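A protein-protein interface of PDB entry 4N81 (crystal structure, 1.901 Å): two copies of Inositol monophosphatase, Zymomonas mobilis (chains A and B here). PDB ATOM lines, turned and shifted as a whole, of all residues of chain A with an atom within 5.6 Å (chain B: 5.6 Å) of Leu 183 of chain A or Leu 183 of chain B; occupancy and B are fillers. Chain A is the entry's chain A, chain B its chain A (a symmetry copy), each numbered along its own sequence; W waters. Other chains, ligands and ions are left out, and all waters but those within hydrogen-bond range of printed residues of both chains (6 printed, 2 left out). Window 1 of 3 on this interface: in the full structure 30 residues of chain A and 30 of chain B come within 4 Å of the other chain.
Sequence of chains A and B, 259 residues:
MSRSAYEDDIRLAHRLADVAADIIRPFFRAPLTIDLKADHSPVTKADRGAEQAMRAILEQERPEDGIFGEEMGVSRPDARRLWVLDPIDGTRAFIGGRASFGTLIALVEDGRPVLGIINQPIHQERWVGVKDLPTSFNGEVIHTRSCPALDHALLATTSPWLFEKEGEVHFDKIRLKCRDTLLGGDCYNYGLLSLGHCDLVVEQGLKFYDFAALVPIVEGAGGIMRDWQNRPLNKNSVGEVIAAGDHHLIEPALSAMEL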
ATOM      1  N   ARG A  98     -14.565  14.234 -14.474  1.00  0.00           N
ATOM      2  CA  ARG A  98     -14.778  13.159 -15.451  1.00  0.00           C
ATOM      3  C   ARG A  98     -14.090  11.873 -15.103  1.00  0.00           C
ATOM      4  O   ARG A  98     -12.919  11.884 -14.729  1.00  0.00           O
ATOM      5  CB  ARG A  98     -14.210  13.562 -16.821  1.00  0.00           C
ATOM      6  CG  ARG A  98     -14.871  14.887 -17.369  1.00  0.00           C
ATOM      7  CD  ARG A  98     -14.155  15.247 -18.698  1.00  0.00           C
ATOM      8  NE  ARG A  98     -14.923  16.260 -19.461  1.00  0.00           N
ATOM      9  CZ  ARG A  98     -14.755  16.418 -20.776  1.00  0.00           C
ATOM     10  NH1 ARG A  98     -13.869  15.647 -21.427  1.00  0.00           N
ATOM     11  NH2 ARG A  98     -15.465  17.336 -21.425  1.00  0.00           N
ATOM     12  N   ALA A 156      -8.901   9.535 -32.207  1.00  0.00           N
ATOM     13  CA  ALA A 156      -9.133  10.258 -30.958  1.00  0.00           C
ATOM     14  C   ALA A 156      -7.866  10.989 -30.609  1.00  0.00           C
ATOM     15  O   ALA A 156      -6.739  10.556 -30.963  1.00  0.00           O
ATOM     16  CB  ALA A 156      -9.452   9.243 -29.789  1.00  0.00           C
ATOM     17  N   THR A 157      -8.040  12.081 -29.878  1.00  0.00           N
ATOM     18  CA  THR A 157      -6.864  12.742 -29.267  1.00  0.00           C
ATOM     19  C   THR A 157      -7.374  13.552 -28.061  1.00  0.00           C
ATOM     20  O   THR A 157      -8.567  13.889 -28.014  1.00  0.00           O
ATOM     21  CB  THR A 157      -6.143  13.708 -30.216  1.00  0.00           C
ATOM     22  OG1 THR A 157      -4.815  13.996 -29.685  1.00  0.00           O
ATOM     23  CG2 THR A 157      -6.930  15.061 -30.406  1.00  0.00           C
ATOM     24  N   THR A 158      -6.507  13.819 -27.089  1.00  0.00           N
ATOM     25  CA  THR A 158      -7.035  14.486 -25.888  1.00  0.00           C
ATOM     26  C   THR A 158      -7.434  15.925 -26.222  1.00  0.00           C
ATOM     27  O   THR A 158      -8.529  16.373 -25.843  1.00  0.00           O
ATOM     28  CB  THR A 158      -5.996  14.466 -24.730  1.00  0.00           C
ATOM     29  OG1 THR A 158      -5.806  13.091 -24.337  1.00  0.00           O
ATOM     30  CG2 THR A 158      -6.546  15.267 -23.536  1.00  0.00           C
ATOM     31  N   SER A 159      -6.556  16.634 -26.943  1.00  0.00           N
ATOM     32  CA  SER A 159      -6.875  18.011 -27.369  1.00  0.00           C
ATOM     33  C   SER A 159      -6.005  18.477 -28.537  1.00  0.00           C
ATOM     34  O   SER A 159      -4.809  18.277 -28.503  1.00  0.00           O
ATOM     35  CB  SER A 159      -6.693  19.001 -26.177  1.00  0.00           C
ATOM     36  OG  SER A 159      -6.876  20.359 -26.640  1.00  0.00           O
ATOM     37  N   PRO A 160      -6.586  19.159 -29.545  1.00  0.00           N
ATOM     38  CA  PRO A 160      -5.761  19.785 -30.588  1.00  0.00           C
ATOM     39  C   PRO A 160      -4.785  20.795 -30.023  1.00  0.00           C
ATOM     40  O   PRO A 160      -3.685  20.988 -30.561  1.00  0.00           O
ATOM     41  CB  PRO A 160      -6.782  20.412 -31.536  1.00  0.00           C
ATOM     42  CG  PRO A 160      -7.959  20.595 -30.761  1.00  0.00           C
ATOM     43  CD  PRO A 160      -8.009  19.449 -29.763  1.00  0.00           C
ATOM     44  N   TRP A 161      -5.159  21.420 -28.917  1.00  0.00           N
ATOM     45  CA  TRP A 161      -4.296  22.448 -28.350  1.00  0.00           C
ATOM     46  C   TRP A 161      -3.171  21.907 -27.467  1.00  0.00           C
ATOM     47  O   TRP A 161      -2.376  22.690 -26.930  1.00  0.00           O
ATOM     48  CB  TRP A 161      -5.144  23.542 -27.647  1.00  0.00           C
ATOM     49  CG  TRP A 161      -6.218  24.019 -28.583  1.00  0.00           C
ATOM     50  CD1 TRP A 161      -6.037  24.684 -29.750  1.00  0.00           C
ATOM     51  CD2 TRP A 161      -7.636  23.821 -28.450  1.00  0.00           C
ATOM     52  NE1 TRP A 161      -7.256  24.932 -30.348  1.00  0.00           N
ATOM     53  CE2 TRP A 161      -8.249  24.427 -29.553  1.00  0.00           C
ATOM     54  CE3 TRP A 161      -8.441  23.233 -27.477  1.00  0.00           C
ATOM     55  CZ2 TRP A 161      -9.642  24.437 -29.729  1.00  0.00           C
ATOM     56  CZ3 TRP A 161      -9.830  23.250 -27.665  1.00  0.00           C
ATOM     57  CH2 TRP A 161     -10.394  23.833 -28.771  1.00  0.00           C
ATOM     58  N   PHE A 171      -1.831  17.099 -37.028  1.00  0.00           N
ATOM     59  CA  PHE A 171      -3.032  16.470 -36.504  1.00  0.00           C
ATOM     60  C   PHE A 171      -4.237  16.849 -37.352  1.00  0.00           C
ATOM     61  O   PHE A 171      -5.098  16.013 -37.673  1.00  0.00           O
ATOM     62  CB  PHE A 171      -3.314  16.830 -35.045  1.00  0.00           C
ATOM     63  CG  PHE A 171      -4.544  16.115 -34.525  1.00  0.00           C
ATOM     64  CD1 PHE A 171      -4.463  14.763 -34.233  1.00  0.00           C
ATOM     65  CD2 PHE A 171      -5.789  16.767 -34.442  1.00  0.00           C
ATOM     66  CE1 PHE A 171      -5.595  14.062 -33.822  1.00  0.00           C
ATOM     67  CE2 PHE A 171      -6.927  16.065 -34.027  1.00  0.00           C
ATOM     68  CZ  PHE A 171      -6.824  14.709 -33.748  1.00  0.00           C
ATOM     69  N   THR A 181     -13.669  12.137 -35.405  1.00  0.00           N
ATOM     70  CA  THR A 181     -12.627  12.344 -34.392  1.00  0.00           C
ATOM     71  C   THR A 181     -13.293  12.580 -33.043  1.00  0.00           C
ATOM     72  O   THR A 181     -14.218  13.417 -32.965  1.00  0.00           O
ATOM     73  CB  THR A 181     -11.773  13.591 -34.798  1.00  0.00           C
ATOM     74  OG1 THR A 181     -11.091  13.289 -36.033  1.00  0.00           O
ATOM     75  CG2 THR A 181     -10.726  13.886 -33.749  1.00  0.00           C
ATOM     76  N   LEU A 182     -12.861  11.878 -31.995  1.00  0.00           N
ATOM     77  CA  LEU A 182     -13.453  12.139 -30.680  1.00  0.00           C
ATOM     78  C   LEU A 182     -12.370  12.779 -29.852  1.00  0.00           C
ATOM     79  O   LEU A 182     -11.178  12.512 -30.063  1.00  0.00           O
ATOM     80  CB  LEU A 182     -13.887  10.845 -30.007  1.00  0.00           C
ATOM     81  CG  LEU A 182     -15.250  10.298 -30.522  1.00  0.00           C
ATOM     82  CD1 LEU A 182     -15.547   8.940 -29.841  1.00  0.00           C
ATOM     83  CD2 LEU A 182     -16.411  11.333 -30.264  1.00  0.00           C
ATOM     84  N   LEU A 183     -12.778  13.637 -28.926  1.00  0.00           N
ATOM     85  CA  LEU A 183     -11.808  14.453 -28.204  1.00  0.00           C
ATOM     86  C   LEU A 183     -11.872  14.231 -26.702  1.00  0.00           C
ATOM     87  O   LEU A 183     -12.908  13.829 -26.171  1.00  0.00           O
ATOM     88  CB  LEU A 183     -12.102  15.945 -28.514  1.00  0.00           C
ATOM     89  CG  LEU A 183     -11.929  16.282 -30.018  1.00  0.00           C
ATOM     90  CD1 LEU A 183     -12.417  17.718 -30.246  1.00  0.00           C
ATOM     91  CD2 LEU A 183     -10.431  16.109 -30.431  1.00  0.00           C
ATOM     92  N   GLY A 184     -10.766  14.493 -26.027  1.00  0.00           N
ATOM     93  CA  GLY A 184     -10.633  14.306 -24.575  1.00  0.00           C
ATOM     94  C   GLY A 184     -10.326  12.855 -24.252  1.00  0.00           C
ATOM     95  O   GLY A 184     -10.641  11.955 -25.040  1.00  0.00           O
ATOM     96  N   GLY A 185      -9.724  12.599 -23.100  1.00  0.00           N
ATOM     97  CA  GLY A 185      -9.736  11.230 -22.578  1.00  0.00           C
ATOM     98  C   GLY A 185      -8.392  10.660 -22.137  1.00  0.00           C
ATOM     99  O   GLY A 185      -8.396   9.699 -21.358  1.00  0.00           O
ATOM    100  N   ASN A 189      -8.503   6.709 -24.157  1.00  0.00           N
ATOM    101  CA  ASN A 189      -8.735   6.388 -25.591  1.00  0.00           C
ATOM    102  C   ASN A 189      -7.926   5.193 -26.047  1.00  0.00           C
ATOM    103  O   ASN A 189      -8.339   4.450 -26.949  1.00  0.00           O
ATOM    104  CB  ASN A 189      -8.414   7.589 -26.478  1.00  0.00           C
ATOM    105  CG  ASN A 189      -9.398   8.724 -26.238  1.00  0.00           C
ATOM    106  OD1 ASN A 189     -10.604   8.515 -26.245  1.00  0.00           O
ATOM    107  ND2 ASN A 189      -8.877   9.914 -26.022  1.00  0.00           N
ATOM    108  N   ARG B  98     -18.011   5.362 -25.558  1.00  0.00           N
ATOM    109  CA  ARG B  98     -17.916   6.219 -24.370  1.00  0.00           C
ATOM    110  C   ARG B  98     -19.213   6.394 -23.640  1.00  0.00           C
ATOM    111  O   ARG B  98     -20.242   6.642 -24.265  1.00  0.00           O
ATOM    112  CB  ARG B  98     -17.484   7.639 -24.771  1.00  0.00           C
ATOM    113  CG  ARG B  98     -16.093   7.647 -25.516  1.00  0.00           C
ATOM    114  CD  ARG B  98     -15.811   9.108 -25.956  1.00  0.00           C
ATOM    115  NE  ARG B  98     -14.390   9.284 -26.346  1.00  0.00           N
ATOM    116  CZ  ARG B  98     -13.812  10.487 -26.352  1.00  0.00           C
ATOM    117  NH1 ARG B  98     -14.528  11.566 -26.002  1.00  0.00           N
ATOM    118  NH2 ARG B  98     -12.536  10.601 -26.707  1.00  0.00           N
ATOM    119  N   ALA B 156     -16.037  23.989 -21.350  1.00  0.00           N
ATOM    120  CA  ALA B 156     -16.106  22.717 -22.065  1.00  0.00           C
ATOM    121  C   ALA B 156     -16.841  22.954 -23.355  1.00  0.00           C
ATOM    122  O   ALA B 156     -17.710  23.858 -23.458  1.00  0.00           O
ATOM    123  CB  ALA B 156     -16.924  21.659 -21.221  1.00  0.00           C
ATOM    124  N   THR B 157     -16.528  22.118 -24.333  1.00  0.00           N
ATOM    125  CA  THR B 157     -17.355  22.092 -25.561  1.00  0.00           C
ATOM    126  C   THR B 157     -17.158  20.712 -26.213  1.00  0.00           C
ATOM    127  O   THR B 157     -16.143  20.052 -25.946  1.00  0.00           O
ATOM    128  CB  THR B 157     -16.960  23.161 -26.587  1.00  0.00           C
ATOM    129  OG1 THR B 157     -18.043  23.320 -27.553  1.00  0.00           O
ATOM    130  CG2 THR B 157     -15.632  22.794 -27.356  1.00  0.00           C
ATOM    131  N   THR B 158     -18.124  20.265 -27.010  1.00  0.00           N
ATOM    132  CA  THR B 158     -17.981  18.895 -27.529  1.00  0.00           C
ATOM    133  C   THR B 158     -16.827  18.833 -28.532  1.00  0.00           C
ATOM    134  O   THR B 158     -15.986  17.921 -28.461  1.00  0.00           O
ATOM    135  CB  THR B 158     -19.301  18.404 -28.190  1.00  0.00           C
ATOM    136  OG1 THR B 158     -20.299  18.304 -27.152  1.00  0.00           O
ATOM    137  CG2 THR B 158     -19.074  17.014 -28.812  1.00  0.00           C
ATOM    138  N   SER B 159     -16.782  19.809 -29.447  1.00  0.00           N
ATOM    139  CA  SER B 159     -15.672  19.873 -30.419  1.00  0.00           C
ATOM    140  C   SER B 159     -15.526  21.259 -31.050  1.00  0.00           C
ATOM    141  O   SER B 159     -16.516  21.835 -31.450  1.00  0.00           O
ATOM    142  CB  SER B 159     -15.887  18.822 -31.553  1.00  0.00           C
ATOM    143  OG  SER B 159     -14.870  18.987 -32.568  1.00  0.00           O
ATOM    144  N   PRO B 160     -14.289  21.773 -31.204  1.00  0.00           N
ATOM    145  CA  PRO B 160     -14.092  23.011 -31.971  1.00  0.00           C
ATOM    146  C   PRO B 160     -14.582  22.890 -33.398  1.00  0.00           C
ATOM    147  O   PRO B 160     -15.037  23.872 -34.002  1.00  0.00           O
ATOM    148  CB  PRO B 160     -12.589  23.264 -31.877  1.00  0.00           C
ATOM    149  CG  PRO B 160     -12.005  21.998 -31.601  1.00  0.00           C
ATOM    150  CD  PRO B 160     -13.003  21.234 -30.744  1.00  0.00           C
ATOM    151  N   TRP B 161     -14.526  21.682 -33.938  1.00  0.00           N
ATOM    152  CA  TRP B 161     -14.926  21.502 -35.327  1.00  0.00           C
ATOM    153  C   TRP B 161     -16.432  21.345 -35.535  1.00  0.00           C
ATOM    154  O   TRP B 161     -16.886  21.184 -36.675  1.00  0.00           O
ATOM    155  CB  TRP B 161     -14.104  20.359 -35.985  1.00  0.00           C
ATOM    156  CG  TRP B 161     -12.640  20.593 -35.738  1.00  0.00           C
ATOM    157  CD1 TRP B 161     -11.893  21.620 -36.214  1.00  0.00           C
ATOM    158  CD2 TRP B 161     -11.761  19.806 -34.916  1.00  0.00           C
ATOM    159  NE1 TRP B 161     -10.595  21.514 -35.755  1.00  0.00           N
ATOM    160  CE2 TRP B 161     -10.493  20.395 -34.973  1.00  0.00           C
ATOM    161  CE3 TRP B 161     -11.922  18.634 -34.179  1.00  0.00           C
ATOM    162  CZ2 TRP B 161      -9.385  19.866 -34.292  1.00  0.00           C
ATOM    163  CZ3 TRP B 161     -10.808  18.116 -33.505  1.00  0.00           C
ATOM    164  CH2 TRP B 161      -9.585  18.734 -33.565  1.00  0.00           C
ATOM    165  N   PHE B 171     -15.226  30.798 -30.483  1.00  0.00           N
ATOM    166  CA  PHE B 171     -14.902  29.825 -29.452  1.00  0.00           C
ATOM    167  C   PHE B 171     -13.432  29.929 -29.073  1.00  0.00           C
ATOM    168  O   PHE B 171     -13.059  29.877 -27.889  1.00  0.00           O
ATOM    169  CB  PHE B 171     -15.212  28.386 -29.863  1.00  0.00           C
ATOM    170  CG  PHE B 171     -14.908  27.412 -28.743  1.00  0.00           C
ATOM    171  CD1 PHE B 171     -15.767  27.345 -27.658  1.00  0.00           C
ATOM    172  CD2 PHE B 171     -13.718  26.660 -28.730  1.00  0.00           C
ATOM    173  CE1 PHE B 171     -15.476  26.513 -26.579  1.00  0.00           C
ATOM    174  CE2 PHE B 171     -13.425  25.821 -27.648  1.00  0.00           C
ATOM    175  CZ  PHE B 171     -14.296  25.778 -26.569  1.00  0.00           C
ATOM    176  N   THR B 181      -9.757  24.145 -20.828  1.00  0.00           N
ATOM    177  CA  THR B 181     -10.898  23.754 -21.664  1.00  0.00           C
ATOM    178  C   THR B 181     -10.936  22.236 -21.767  1.00  0.00           C
ATOM    179  O   THR B 181      -9.887  21.625 -22.066  1.00  0.00           O
ATOM    180  CB  THR B 181     -10.722  24.389 -23.084  1.00  0.00           C
ATOM    181  OG1 THR B 181     -10.782  25.824 -22.948  1.00  0.00           O
ATOM    182  CG2 THR B 181     -11.842  23.959 -24.003  1.00  0.00           C
ATOM    183  N   LEU B 182     -12.093  21.615 -21.532  1.00  0.00           N
ATOM    184  CA  LEU B 182     -12.156  20.160 -21.687  1.00  0.00           C
ATOM    185  C   LEU B 182     -13.030  19.904 -22.886  1.00  0.00           C
ATOM    186  O   LEU B 182     -13.932  20.698 -23.188  1.00  0.00           O
ATOM    187  CB  LEU B 182     -12.790  19.506 -20.468  1.00  0.00           C
ATOM    188  CG  LEU B 182     -11.816  19.345 -19.265  1.00  0.00           C
ATOM    189  CD1 LEU B 182     -12.585  18.758 -18.058  1.00  0.00           C
ATOM    190  CD2 LEU B 182     -10.583  18.441 -19.652  1.00  0.00           C
ATOM    191  N   LEU B 183     -12.751  18.810 -23.583  1.00  0.00           N
ATOM    192  CA  LEU B 183     -13.405  18.570 -24.865  1.00  0.00           C
ATOM    193  C   LEU B 183     -14.179  17.262 -24.883  1.00  0.00           C
ATOM    194  O   LEU B 183     -13.869  16.340 -24.127  1.00  0.00           O
ATOM    195  CB  LEU B 183     -12.312  18.532 -25.968  1.00  0.00           C
ATOM    196  CG  LEU B 183     -11.561  19.882 -26.102  1.00  0.00           C
ATOM    197  CD1 LEU B 183     -10.393  19.685 -27.076  1.00  0.00           C
ATOM    198  CD2 LEU B 183     -12.546  20.992 -26.597  1.00  0.00           C
ATOM    199  N   GLY B 184     -15.181  17.191 -25.743  1.00  0.00           N
ATOM    200  CA  GLY B 184     -16.058  16.019 -25.875  1.00  0.00           C
ATOM    201  C   GLY B 184     -17.145  16.047 -24.816  1.00  0.00           C
ATOM    202  O   GLY B 184     -16.981  16.672 -23.762  1.00  0.00           O
ATOM    203  N   GLY B 185     -18.258  15.371 -25.064  1.00  0.00           N
ATOM    204  CA  GLY B 185     -19.167  15.063 -23.956  1.00  0.00           C
ATOM    205  C   GLY B 185     -20.639  15.400 -24.171  1.00  0.00           C
ATOM    206  O   GLY B 185     -21.476  14.828 -23.462  1.00  0.00           O
ATOM    207  N   ASN B 189     -21.530  17.523 -20.377  1.00  0.00           N
ATOM    208  CA  ASN B 189     -20.837  18.685 -19.760  1.00  0.00           C
ATOM    209  C   ASN B 189     -21.796  19.605 -19.036  1.00  0.00           C
ATOM    210  O   ASN B 189     -21.429  20.265 -18.054  1.00  0.00           O
ATOM    211  CB  ASN B 189     -20.063  19.479 -20.810  1.00  0.00           C
ATOM    212  CG  ASN B 189     -18.902  18.668 -21.365  1.00  0.00           C
ATOM    213  OD1 ASN B 189     -18.119  18.107 -20.610  1.00  0.00           O
ATOM    214  ND2 ASN B 189     -18.804  18.606 -22.676  1.00  0.00           N
HETATM  215  O   HOH W   1     -16.233  18.683 -18.621  1.00  0.00           O
HETATM  216  O   HOH W   2     -14.407  16.447 -33.442  1.00  0.00           O
HETATM  217  O   HOH W   3      -8.041  21.616 -24.522  1.00  0.00           O
HETATM  218  O   HOH W   4     -17.922  15.070 -20.617  1.00  0.00           O
HETATM  219  O   HOH W   5     -12.646   7.653 -27.956  1.00  0.00           O
HETATM  220  O   HOH W   6     -12.229   8.947 -23.708  1.00  0.00           O
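Of the 14 printed residues of chain B, 10 touch a printed residue of chain A. Hydrophobic or aromatic side chains of chain B within 4 Å of the printed part of chain A: Pro 160, Trp 161, Phe 171, Leu 182 and Leu 183. Of the 14 printed residues of chain A, 10 touch a printed residue of chain B. Printed residues of chain A that touch a printed residue of chain B: Arg 98, Thr 158, Ser 159, Pro 160, Trp 161, Phe 171, Leu 182, Leu 183, Gly 184 and Asn 189. Among the printed residues, 23 pairs touch across the chains. Among the printed residues, no Asp or Glu carboxylate lies within 4 Å of a Lys or Arg side-chain nitrogen of the other chain.
Arg 98 of chain A touches Leu 182 of chain B, and with the chains exchanged Leu 182 of chain A touches Arg 98 of chain B. Trp 161 of chain A touches Phe 171 of chain B, and with the chains exchanged Phe 171 of chain A touches Trp 161 of chain B. Trp 161 of chain A touches Leu 183 of chain B, and with the chains exchanged Leu 183 of chain A touches Trp 161 of chain B. Leu 183 of chain A touches its own counterpart, Leu 183 of chain B. Positions printed for both chains: 98, 156, 157, 158, 159, 160, 161, 171, 181, 182, 183, 184, 185 and 189.
N of Thr 157 of chain A is in hydrogen-bond range of O of Leu 182 of chain A (3.2 Å). The backbone carbonyl oxygen (O) of Thr 157 of chain A lies within hydrogen-bond range of the backbone NH (N) of Gly 184 of chain A, at 3.0 Å. The backbone NH of Gly 184 of chain A sits at hydrogen-bond distance from the backbone carbonyl oxygen of Thr 158 of chain A, 2.9 Å away. N of Gly 184 of chain B is in hydrogen-bond range of O of Thr 157 of chain B (3.0 Å). The backbone carbonyl oxygen of Thr 158 of chain B lies within hydrogen-bond range of the backbone NH of Gly 184 of chain B (2.9 Å). The backbone carbonyl oxygen of Gly 184 of chain B sits at hydrogen-bond distance from the side-chain amide nitrogen of Asn 189 of chain B, 2.9 Å away.
Water W3 lies within hydrogen-bond range of the side-chain hydroxyl of Ser 159 of chain A (2.7 Å) and the backbone carbonyl oxygen of Thr 181 of chain B (3.1 Å). Water W2 bridges the side-chain hydroxyl (OG) of Ser 159 of chain B and the backbone carbonyl oxygen (O) of Thr 181 of chain A. Water W1 lies within hydrogen-bond range of the side-chain amide oxygen of Asn 189 of chain B (2.8 Å) and the guanidinium group of Arg 98 of chain A (2.9 Å). Water W5 lies within hydrogen-bond range of OD1 of Asn 189 of chain A (2.8 Å) and NE of Arg 98 of chain B (2.9 Å). Water W6 lies within hydrogen-bond range of the side-chain amide oxygen (OD1) of Asn 189 of chain A and the guanidinium group (NE) of Arg 98 of chain B. Water W4 bridges OD1 of Asn 189 of chain B (3.0 Å) and NE of Arg 98 of chain A (3.4 Å).
Among the printed residues, pairs that only touch across the chains: Arg 98 of chain A with Leu 182 of chain B, Thr 158 of chain A with Leu 183 of chain B, Ser 159 of chain A with Leu 183 of chain B, Pro 160 of chain A with Trp 161 of chain B, Pro 160 of chain A with Leu 183 of chain B, Trp 161 of chain A with Pro 160 of chain B, Trp 161 of chain A with Phe 171 of chain B, Trp 161 of chain A with Leu 183 of chain B, Phe 171 of chain A with Trp 161 of chain B, Leu 182 of chain A with Arg 98 of chain B, Leu 183 of chain A with Thr 158 of chain B, Leu 183 of chain A with Ser 159 of chain B, Leu 183 of chain A with Pro 160 of chain B, Leu 183 of chain A with Trp 161 of chain B, Leu 183 of chain A with Gly 184 of chain B and Gly 184 of chain A with Leu 183 of chain B.
The guanidinium group (NH1) of Arg 98 of chain A sits at hydrogen-bond distance from the backbone carbonyl oxygen (O) of Leu 183 of chain B (2.8 Å). The guanidinium group (NH2) of Arg 98 of chain A is in hydrogen-bond range of the backbone carbonyl oxygen (O) of Gly 184 of chain B (2.9 Å). The side-chain amide oxygen of Asn 189 of chain B sits at hydrogen-bond distance from the guanidinium group of Arg 98 of chain A, 2.9 Å away. O of Leu 183 of chain A sits at hydrogen-bond distance from NH1 of Arg 98 of chain B (2.8 Å). O of Gly 184 of chain A is in hydrogen-bond range of NH2 of Arg 98 of chain B (2.9 Å). NH2 of Arg 98 of chain B sits at hydrogen-bond distance from OD1 of Asn 189 of chain A, 2.9 Å away. O of Leu 183 of chain B sits close to O of Leu 183 of chain A (3.4 Å).
Of the printed residues of chain B, Leu 183 of chain A touches Arg 98, Thr 158, Ser 159, Pro 160, Trp 161, Leu 183 and Gly 184. Printed residues of chain B within 4 Å of Arg 98 of chain A: Leu 182, Leu 183, Gly 184 and Asn 189. Of the printed residues of chain A, Phe 171 of chain B touches Trp 161. Printed residues of chain B within 4 Å of Phe 171 of chain A: Trp 161. The nearest printed residue of chain B that does not touch Leu 183 of chain A is Gly 185 of chain B (5.7 Å). The nearest printed residue of chain A that does not touch Leu 183 of chain B is Gly 185 of chain A (5.7 Å). The nearest printed residue of chain B that does not touch Leu 182 of chain A is Gly 184 of chain B (6.3 Å).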
